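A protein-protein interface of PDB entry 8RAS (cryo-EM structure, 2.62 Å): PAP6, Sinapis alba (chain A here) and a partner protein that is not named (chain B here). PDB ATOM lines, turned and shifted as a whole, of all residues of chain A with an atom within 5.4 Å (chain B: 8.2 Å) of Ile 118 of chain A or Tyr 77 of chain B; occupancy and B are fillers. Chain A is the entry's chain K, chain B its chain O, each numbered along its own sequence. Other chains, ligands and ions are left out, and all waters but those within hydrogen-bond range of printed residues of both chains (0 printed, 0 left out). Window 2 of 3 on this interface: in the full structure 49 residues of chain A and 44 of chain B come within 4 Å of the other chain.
O of His 115 of chain A touches CG2 of Thr 106 of chain B, at 3.99 Å.
Tyr 77 of chain B touches Asp 117 of chain A.
Asp 117 of chain A touches Val 79 of chain B (OD1 to O, 3.8 Å).
Ile 118 of chain A touches Tyr 77 of chain B (CA to OH, 3.5 Å).
Tyr 119 of chain A touches Ile 112 of chain B (CB to CG2, 3.7 Å).
Tyr 119 of chain A touches Gln 116 of chain B.
CD2 of Tyr 104 of chain B touches CH2 of Trp 122 of chain A (3.7 Å).
Trp 122 of chain A touches Thr 106 of chain B.
Ile 112 of chain B touches Trp 122 of chain A.
Of the 8 printed residues of chain A, 6 touch a printed residue of chain B.
Printed residues of chain A that touch a printed residue of chain B: His 115, Pro 116, Asp 117, Ile 118, Tyr 119 and Trp 122.
Hydrophobic or aromatic side chains of chain A that line the printed part of chain B: Pro 116, Ile 118, Tyr 119 and Trp 122.
Printed residues of chain B that touch a printed residue of chain A: Tyr 77, Val 79, Tyr 104, Thr 106, Ile 112, Gln 116 and Lys 133.
Along chain B the printed residues that touch a printed residue of chain A span positions 77 to 133.
Among the printed residues, 12 pairs touch across the chains.
ND1 of His 115 of chain A is in hydrogen-bond range of N of Asp 117 of chain A, at 3.0 Å.
ND1 of His 115 of chain A is in hydrogen-bond range of N of Ile 118 of chain A (3.2 Å).
The indole nitrogen (NE1) of Trp 122 of chain A lies within hydrogen-bond range of the backbone carbonyl oxygen (O) of His 115 of chain A (2.6 Å).
The backbone carbonyl oxygen (O) of Tyr 77 of chain B is in hydrogen-bond range of the guanidinium group (NH1) of Arg 80 of chain B (3.4 Å).
N of Val 79 of chain B sits at hydrogen-bond distance from OE2 of Glu 119 of chain B (3.3 Å).
The backbone carbonyl oxygen (O) of Arg 80 of chain B sits at hydrogen-bond distance from the backbone NH (N) of Lys 133 of chain B (3.0 Å).
The backbone carbonyl oxygen (O) of Pro 116 of chain A is in hydrogen-bond range of the side-chain hydroxyl (OH) of Tyr 104 of chain B (3.4 Å).
The backbone carbonyl oxygen (O) of Pro 116 of chain A sits at hydrogen-bond distance from the side-chain amino group (NZ) of Lys 133 of chain B (3.0 Å).
The side-chain carboxylate (OD1) of Asp 117 of chain A lies close to the side-chain amino group (NZ) of Lys 133 of chain B, at 2.4 Å.
Ile 118 of chain A touches one residue of chain B.
Of the printed residues of chain A, Tyr 77 of chain B touches Asp 117 and Ile 118.
Of the printed residues of chain A, Thr 106 of chain B touches His 115 and Trp 122.
Printed residues of chain B within 4 Å of Tyr 119 of chain A: Ile 112 and Gln 116.
The nearest residue of chain B that does not touch Ile 118 of chain A is Lys 133 of chain B (6.0 Å).
The nearest printed residue of chain B that does not touch Trp 122 of chain A is Ala 115 of chain B (4.4 Å).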
ATOM      1  N   HIS A 115     -23.340 -35.792  17.856  1.00  0.00           N
ATOM      2  CA  HIS A 115     -24.503 -35.343  18.608  1.00  0.00           C
ATOM      3  C   HIS A 115     -25.609 -34.917  17.648  1.00  0.00           C
ATOM      4  O   HIS A 115     -25.339 -34.179  16.689  1.00  0.00           O
ATOM      5  CB  HIS A 115     -24.129 -34.187  19.533  1.00  0.00           C
ATOM      6  CG  HIS A 115     -25.128 -33.934  20.617  1.00  0.00           C
ATOM      7  ND1 HIS A 115     -26.325 -33.290  20.391  1.00  0.00           N
ATOM      8  CD2 HIS A 115     -25.109 -34.240  21.935  1.00  0.00           C
ATOM      9  CE1 HIS A 115     -27.000 -33.209  21.523  1.00  0.00           C
ATOM     10  NE2 HIS A 115     -26.284 -33.779  22.475  1.00  0.00           N
ATOM     11  N   PRO A 116     -26.850 -35.361  17.856  1.00  0.00           N
ATOM     12  CA  PRO A 116     -27.924 -35.016  16.912  1.00  0.00           C
ATOM     13  C   PRO A 116     -28.217 -33.530  16.822  1.00  0.00           C
ATOM     14  O   PRO A 116     -28.748 -33.083  15.799  1.00  0.00           O
ATOM     15  CB  PRO A 116     -29.133 -35.791  17.454  1.00  0.00           C
ATOM     16  CG  PRO A 116     -28.799 -36.088  18.874  1.00  0.00           C
ATOM     17  CD  PRO A 116     -27.318 -36.259  18.924  1.00  0.00           C
ATOM     18  N   ASP A 117     -27.892 -32.749  17.849  1.00  0.00           N
ATOM     19  CA  ASP A 117     -28.213 -31.327  17.883  1.00  0.00           C
ATOM     20  C   ASP A 117     -26.999 -30.424  17.759  1.00  0.00           C
ATOM     21  O   ASP A 117     -27.069 -29.397  17.082  1.00  0.00           O
ATOM     22  CB  ASP A 117     -28.954 -30.986  19.179  1.00  0.00           C
ATOM     23  CG  ASP A 117     -30.357 -31.544  19.212  1.00  0.00           C
ATOM     24  OD1 ASP A 117     -31.115 -31.302  18.251  1.00  0.00           O
ATOM     25  OD2 ASP A 117     -30.704 -32.225  20.198  1.00  0.00           O
ATOM     26  N   ILE A 118     -25.885 -30.778  18.393  1.00  0.00           N
ATOM     27  CA  ILE A 118     -24.711 -29.917  18.422  1.00  0.00           C
ATOM     28  C   ILE A 118     -23.938 -30.081  17.121  1.00  0.00           C
ATOM     29  O   ILE A 118     -23.078 -30.960  17.001  1.00  0.00           O
ATOM     30  CB  ILE A 118     -23.832 -30.224  19.647  1.00  0.00           C
ATOM     31  CG1 ILE A 118     -24.649 -30.064  20.930  1.00  0.00           C
ATOM     32  CG2 ILE A 118     -22.622 -29.311  19.686  1.00  0.00           C
ATOM     33  CD1 ILE A 118     -23.945 -30.544  22.176  1.00  0.00           C
ATOM     34  N   TYR A 119     -24.246 -29.235  16.137  1.00  0.00           N
ATOM     35  CA  TYR A 119     -23.576 -29.298  14.846  1.00  0.00           C
ATOM     36  C   TYR A 119     -22.132 -28.822  14.909  1.00  0.00           C
ATOM     37  O   TYR A 119     -21.404 -28.980  13.923  1.00  0.00           O
ATOM     38  CB  TYR A 119     -24.352 -28.484  13.807  1.00  0.00           C
ATOM     39  CG  TYR A 119     -24.777 -27.117  14.286  1.00  0.00           C
ATOM     40  CD1 TYR A 119     -23.879 -26.058  14.318  1.00  0.00           C
ATOM     41  CD2 TYR A 119     -26.078 -26.883  14.702  1.00  0.00           C
ATOM     42  CE1 TYR A 119     -24.265 -24.811  14.755  1.00  0.00           C
ATOM     43  CE2 TYR A 119     -26.473 -25.640  15.140  1.00  0.00           C
ATOM     44  CZ  TYR A 119     -25.563 -24.608  15.165  1.00  0.00           C
ATOM     45  OH  TYR A 119     -25.955 -23.365  15.602  1.00  0.00           O
ATOM     46  N   SER A 120     -21.706 -28.236  16.028  1.00  0.00           N
ATOM     47  CA  SER A 120     -20.303 -27.881  16.189  1.00  0.00           C
ATOM     48  C   SER A 120     -19.414 -29.110  16.319  1.00  0.00           C
ATOM     49  O   SER A 120     -18.198 -29.005  16.128  1.00  0.00           O
ATOM     50  CB  SER A 120     -20.127 -26.966  17.401  1.00  0.00           C
ATOM     51  OG  SER A 120     -19.990 -27.714  18.595  1.00  0.00           O
ATOM     52  N   GLN A 121     -19.991 -30.270  16.634  1.00  0.00           N
ATOM     53  CA  GLN A 121     -19.248 -31.521  16.671  1.00  0.00           C
ATOM     54  C   GLN A 121     -19.168 -32.209  15.318  1.00  0.00           C
ATOM     55  O   GLN A 121     -18.345 -33.113  15.148  1.00  0.00           O
ATOM     56  CB  GLN A 121     -19.887 -32.493  17.666  1.00  0.00           C
ATOM     57  CG  GLN A 121     -19.885 -32.027  19.101  1.00  0.00           C
ATOM     58  CD  GLN A 121     -20.532 -33.034  20.024  1.00  0.00           C
ATOM     59  OE1 GLN A 121     -20.819 -34.161  19.624  1.00  0.00           O
ATOM     60  NE2 GLN A 121     -20.770 -32.634  21.267  1.00  0.00           N
ATOM     61  N   TRP A 122     -20.000 -31.810  14.357  1.00  0.00           N
ATOM     62  CA  TRP A 122     -20.093 -32.534  13.096  1.00  0.00           C
ATOM     63  C   TRP A 122     -18.885 -32.318  12.198  1.00  0.00           C
ATOM     64  O   TRP A 122     -18.730 -33.048  11.215  1.00  0.00           O
ATOM     65  CB  TRP A 122     -21.373 -32.142  12.354  1.00  0.00           C
ATOM     66  CG  TRP A 122     -22.637 -32.375  13.137  1.00  0.00           C
ATOM     67  CD1 TRP A 122     -22.743 -32.889  14.397  1.00  0.00           C
ATOM     68  CD2 TRP A 122     -23.973 -32.102  12.704  1.00  0.00           C
ATOM     69  NE1 TRP A 122     -24.059 -32.948  14.777  1.00  0.00           N
ATOM     70  CE2 TRP A 122     -24.836 -32.470  13.754  1.00  0.00           C
ATOM     71  CE3 TRP A 122     -24.525 -31.580  11.532  1.00  0.00           C
ATOM     72  CZ2 TRP A 122     -26.217 -32.333  13.667  1.00  0.00           C
ATOM     73  CZ3 TRP A 122     -25.894 -31.445  11.447  1.00  0.00           C
ATOM     74  CH2 TRP A 122     -26.725 -31.820  12.508  1.00  0.00           C
ATOM     75  N   ARG B  74     -33.061 -22.436  29.528  1.00  0.00           N
ATOM     76  CA  ARG B  74     -33.710 -22.713  28.256  1.00  0.00           C
ATOM     77  C   ARG B  74     -32.862 -23.670  27.425  1.00  0.00           C
ATOM     78  O   ARG B  74     -31.631 -23.657  27.485  1.00  0.00           O
ATOM     79  CB  ARG B  74     -33.932 -21.408  27.490  1.00  0.00           C
ATOM     80  CG  ARG B  74     -34.867 -21.496  26.295  1.00  0.00           C
ATOM     81  CD  ARG B  74     -36.238 -22.019  26.680  1.00  0.00           C
ATOM     82  NE  ARG B  74     -37.224 -21.740  25.643  1.00  0.00           N
ATOM     83  CZ  ARG B  74     -37.927 -22.664  25.004  1.00  0.00           C
ATOM     84  NH1 ARG B  74     -37.789 -23.949  25.279  1.00  0.00           N
ATOM     85  NH2 ARG B  74     -38.793 -22.287  24.068  1.00  0.00           N
ATOM     86  N   GLU B  75     -33.533 -24.517  26.649  1.00  0.00           N
ATOM     87  CA  GLU B  75     -32.823 -25.414  25.750  1.00  0.00           C
ATOM     88  C   GLU B  75     -32.310 -24.655  24.532  1.00  0.00           C
ATOM     89  O   GLU B  75     -32.942 -23.713  24.046  1.00  0.00           O
ATOM     90  CB  GLU B  75     -33.718 -26.573  25.311  1.00  0.00           C
ATOM     91  CG  GLU B  75     -35.087 -26.159  24.810  1.00  0.00           C
ATOM     92  CD  GLU B  75     -36.183 -26.482  25.805  1.00  0.00           C
ATOM     93  OE1 GLU B  75     -35.857 -26.840  26.956  1.00  0.00           O
ATOM     94  OE2 GLU B  75     -37.372 -26.378  25.435  1.00  0.00           O
ATOM     95  N   ASP B  76     -31.145 -25.079  24.043  1.00  0.00           N
ATOM     96  CA  ASP B  76     -30.475 -24.372  22.960  1.00  0.00           C
ATOM     97  C   ASP B  76     -31.034 -24.710  21.585  1.00  0.00           C
ATOM     98  O   ASP B  76     -30.750 -23.985  20.625  1.00  0.00           O
ATOM     99  CB  ASP B  76     -28.977 -24.678  22.987  1.00  0.00           C
ATOM    100  CG  ASP B  76     -28.292 -24.123  24.216  1.00  0.00           C
ATOM    101  OD1 ASP B  76     -28.505 -22.934  24.526  1.00  0.00           O
ATOM    102  OD2 ASP B  76     -27.540 -24.872  24.872  1.00  0.00           O
ATOM    103  N   TYR B  77     -31.812 -25.782  21.460  1.00  0.00           N
ATOM    104  CA  TYR B  77     -32.303 -26.238  20.167  1.00  0.00           C
ATOM    105  C   TYR B  77     -33.800 -26.483  20.247  1.00  0.00           C
ATOM    106  O   TYR B  77     -34.278 -27.143  21.176  1.00  0.00           O
ATOM    107  CB  TYR B  77     -31.571 -27.508  19.723  1.00  0.00           C
ATOM    108  CG  TYR B  77     -30.069 -27.358  19.746  1.00  0.00           C
ATOM    109  CD1 TYR B  77     -29.392 -26.800  18.671  1.00  0.00           C
ATOM    110  CD2 TYR B  77     -29.331 -27.756  20.850  1.00  0.00           C
ATOM    111  CE1 TYR B  77     -28.021 -26.652  18.693  1.00  0.00           C
ATOM    112  CE2 TYR B  77     -27.961 -27.613  20.880  1.00  0.00           C
ATOM    113  CZ  TYR B  77     -27.311 -27.061  19.800  1.00  0.00           C
ATOM    114  OH  TYR B  77     -25.944 -26.919  19.828  1.00  0.00           O
ATOM    115  N   LEU B  78     -34.537 -25.952  19.271  1.00  0.00           N
ATOM    116  CA  LEU B  78     -35.986 -26.090  19.231  1.00  0.00           C
ATOM    117  C   LEU B  78     -36.465 -27.166  18.269  1.00  0.00           C
ATOM    118  O   LEU B  78     -37.614 -27.605  18.382  1.00  0.00           O
ATOM    119  CB  LEU B  78     -36.634 -24.755  18.843  1.00  0.00           C
ATOM    120  CG  LEU B  78     -36.367 -23.568  19.768  1.00  0.00           C
ATOM    121  CD1 LEU B  78     -37.112 -22.343  19.278  1.00  0.00           C
ATOM    122  CD2 LEU B  78     -36.759 -23.904  21.195  1.00  0.00           C
ATOM    123  N   VAL B  79     -35.625 -27.596  17.334  1.00  0.00           N
ATOM    124  CA  VAL B  79     -36.008 -28.632  16.382  1.00  0.00           C
ATOM    125  C   VAL B  79     -35.812 -29.993  17.032  1.00  0.00           C
ATOM    126  O   VAL B  79     -34.720 -30.316  17.513  1.00  0.00           O
ATOM    127  CB  VAL B  79     -35.195 -28.507  15.085  1.00  0.00           C
ATOM    128  CG1 VAL B  79     -35.546 -29.631  14.126  1.00  0.00           C
ATOM    129  CG2 VAL B  79     -35.441 -27.155  14.438  1.00  0.00           C
ATOM    130  N   ARG B  80     -36.871 -30.795  17.049  1.00  0.00           N
ATOM    131  CA  ARG B  80     -36.869 -32.086  17.719  1.00  0.00           C
ATOM    132  C   ARG B  80     -36.592 -33.202  16.724  1.00  0.00           C
ATOM    133  O   ARG B  80     -37.054 -33.160  15.581  1.00  0.00           O
ATOM    134  CB  ARG B  80     -38.206 -32.335  18.421  1.00  0.00           C
ATOM    135  CG  ARG B  80     -38.076 -32.646  19.900  1.00  0.00           C
ATOM    136  CD  ARG B  80     -37.389 -31.512  20.639  1.00  0.00           C
ATOM    137  NE  ARG B  80     -38.187 -30.292  20.628  1.00  0.00           N
ATOM    138  CZ  ARG B  80     -37.894 -29.200  21.319  1.00  0.00           C
ATOM    139  NH1 ARG B  80     -36.822 -29.138  22.092  1.00  0.00           N
ATOM    140  NH2 ARG B  80     -38.696 -28.142  21.232  1.00  0.00           N
ATOM    141  N   TYR B 104     -31.443 -35.466   7.512  1.00  0.00           N
ATOM    142  CA  TYR B 104     -30.082 -34.989   7.688  1.00  0.00           C
ATOM    143  C   TYR B 104     -29.190 -36.132   8.143  1.00  0.00           C
ATOM    144  O   TYR B 104     -29.662 -37.168   8.616  1.00  0.00           O
ATOM    145  CB  TYR B 104     -30.018 -33.842   8.702  1.00  0.00           C
ATOM    146  CG  TYR B 104     -30.080 -34.299  10.141  1.00  0.00           C
ATOM    147  CD1 TYR B 104     -31.282 -34.682  10.715  1.00  0.00           C
ATOM    148  CD2 TYR B 104     -28.936 -34.347  10.925  1.00  0.00           C
ATOM    149  CE1 TYR B 104     -31.343 -35.101  12.027  1.00  0.00           C
ATOM    150  CE2 TYR B 104     -28.989 -34.766  12.238  1.00  0.00           C
ATOM    151  CZ  TYR B 104     -30.195 -35.140  12.784  1.00  0.00           C
ATOM    152  OH  TYR B 104     -30.254 -35.557  14.092  1.00  0.00           O
ATOM    153  N   THR B 106     -25.189 -36.383  10.218  1.00  0.00           N
ATOM    154  CA  THR B 106     -24.137 -35.603  10.861  1.00  0.00           C
ATOM    155  C   THR B 106     -22.843 -35.592  10.057  1.00  0.00           C
ATOM    156  O   THR B 106     -22.038 -34.671  10.220  1.00  0.00           O
ATOM    157  CB  THR B 106     -23.872 -36.134  12.269  1.00  0.00           C
ATOM    158  OG1 THR B 106     -23.519 -37.520  12.202  1.00  0.00           O
ATOM    159  CG2 THR B 106     -25.107 -35.974  13.136  1.00  0.00           C
ATOM    160  N   ILE B 112     -25.063 -28.882   8.303  1.00  0.00           N
ATOM    161  CA  ILE B 112     -24.816 -27.938   9.390  1.00  0.00           C
ATOM    162  C   ILE B 112     -25.510 -26.609   9.105  1.00  0.00           C
ATOM    163  O   ILE B 112     -26.219 -26.054   9.960  1.00  0.00           O
ATOM    164  CB  ILE B 112     -23.303 -27.751   9.593  1.00  0.00           C
ATOM    165  CG1 ILE B 112     -22.632 -29.103   9.841  1.00  0.00           C
ATOM    166  CG2 ILE B 112     -23.028 -26.792  10.737  1.00  0.00           C
ATOM    167  CD1 ILE B 112     -21.127 -29.038   9.907  1.00  0.00           C
ATOM    168  N   ALA B 115     -29.107 -27.060   9.408  1.00  0.00           N
ATOM    169  CA  ALA B 115     -29.495 -27.130  10.813  1.00  0.00           C
ATOM    170  C   ALA B 115     -29.659 -25.736  11.405  1.00  0.00           C
ATOM    171  O   ALA B 115     -30.646 -25.450  12.093  1.00  0.00           O
ATOM    172  CB  ALA B 115     -28.464 -27.934  11.604  1.00  0.00           C
ATOM    173  N   GLN B 116     -28.701 -24.847  11.133  1.00  0.00           N
ATOM    174  CA  GLN B 116     -28.814 -23.480  11.639  1.00  0.00           C
ATOM    175  C   GLN B 116     -30.000 -22.749  11.016  1.00  0.00           C
ATOM    176  O   GLN B 116     -30.726 -22.018  11.707  1.00  0.00           O
ATOM    177  CB  GLN B 116     -27.513 -22.725  11.385  1.00  0.00           C
ATOM    178  CG  GLN B 116     -26.283 -23.455  11.890  1.00  0.00           C
ATOM    179  CD  GLN B 116     -25.023 -22.634  11.761  1.00  0.00           C
ATOM    180  OE1 GLN B 116     -24.895 -21.574  12.369  1.00  0.00           O
ATOM    181  NE2 GLN B 116     -24.080 -23.121  10.967  1.00  0.00           N
ATOM    182  N   GLU B 119     -33.128 -23.982  12.652  1.00  0.00           N
ATOM    183  CA  GLU B 119     -33.256 -23.403  13.986  1.00  0.00           C
ATOM    184  C   GLU B 119     -33.800 -21.981  13.911  1.00  0.00           C
ATOM    185  O   GLU B 119     -34.688 -21.601  14.687  1.00  0.00           O
ATOM    186  CB  GLU B 119     -31.908 -23.429  14.702  1.00  0.00           C
ATOM    187  CG  GLU B 119     -31.540 -24.784  15.270  1.00  0.00           C
ATOM    188  CD  GLU B 119     -32.401 -25.171  16.452  1.00  0.00           C
ATOM    189  OE1 GLU B 119     -32.880 -24.263  17.164  1.00  0.00           O
ATOM    190  OE2 GLU B 119     -32.602 -26.382  16.669  1.00  0.00           O
ATOM    191  N   ALA B 122     -37.486 -22.221  13.071  1.00  0.00           N
ATOM    192  CA  ALA B 122     -38.262 -22.618  14.240  1.00  0.00           C
ATOM    193  C   ALA B 122     -38.443 -21.452  15.199  1.00  0.00           C
ATOM    194  O   ALA B 122     -39.510 -21.296  15.803  1.00  0.00           O
ATOM    195  CB  ALA B 122     -37.588 -23.794  14.945  1.00  0.00           C
ATOM    196  N   VAL B 123     -37.407 -20.628  15.363  1.00  0.00           N
ATOM    197  CA  VAL B 123     -37.558 -19.417  16.165  1.00  0.00           C
ATOM    198  C   VAL B 123     -38.593 -18.491  15.538  1.00  0.00           C
ATOM    199  O   VAL B 123     -39.394 -17.862  16.240  1.00  0.00           O
ATOM    200  CB  VAL B 123     -36.199 -18.714  16.342  1.00  0.00           C
ATOM    201  CG1 VAL B 123     -36.383 -17.360  17.002  1.00  0.00           C
ATOM    202  CG2 VAL B 123     -35.260 -19.579  17.163  1.00  0.00           C
ATOM    203  N   LYS B 133     -36.778 -33.262  12.611  1.00  0.00           N
ATOM    204  CA  LYS B 133     -35.655 -33.761  11.834  1.00  0.00           C
ATOM    205  C   LYS B 133     -35.542 -35.268  12.000  1.00  0.00           C
ATOM    206  O   LYS B 133     -35.781 -35.802  13.086  1.00  0.00           O
ATOM    207  CB  LYS B 133     -34.342 -33.089  12.247  1.00  0.00           C
ATOM    208  CG  LYS B 133     -34.061 -33.129  13.734  1.00  0.00           C
ATOM    209  CD  LYS B 133     -32.841 -32.303  14.080  1.00  0.00           C
ATOM    210  CE  LYS B 133     -32.412 -32.537  15.513  1.00  0.00           C
ATOM    211  NZ  LYS B 133     -31.326 -31.609  15.914  1.00  0.00           N
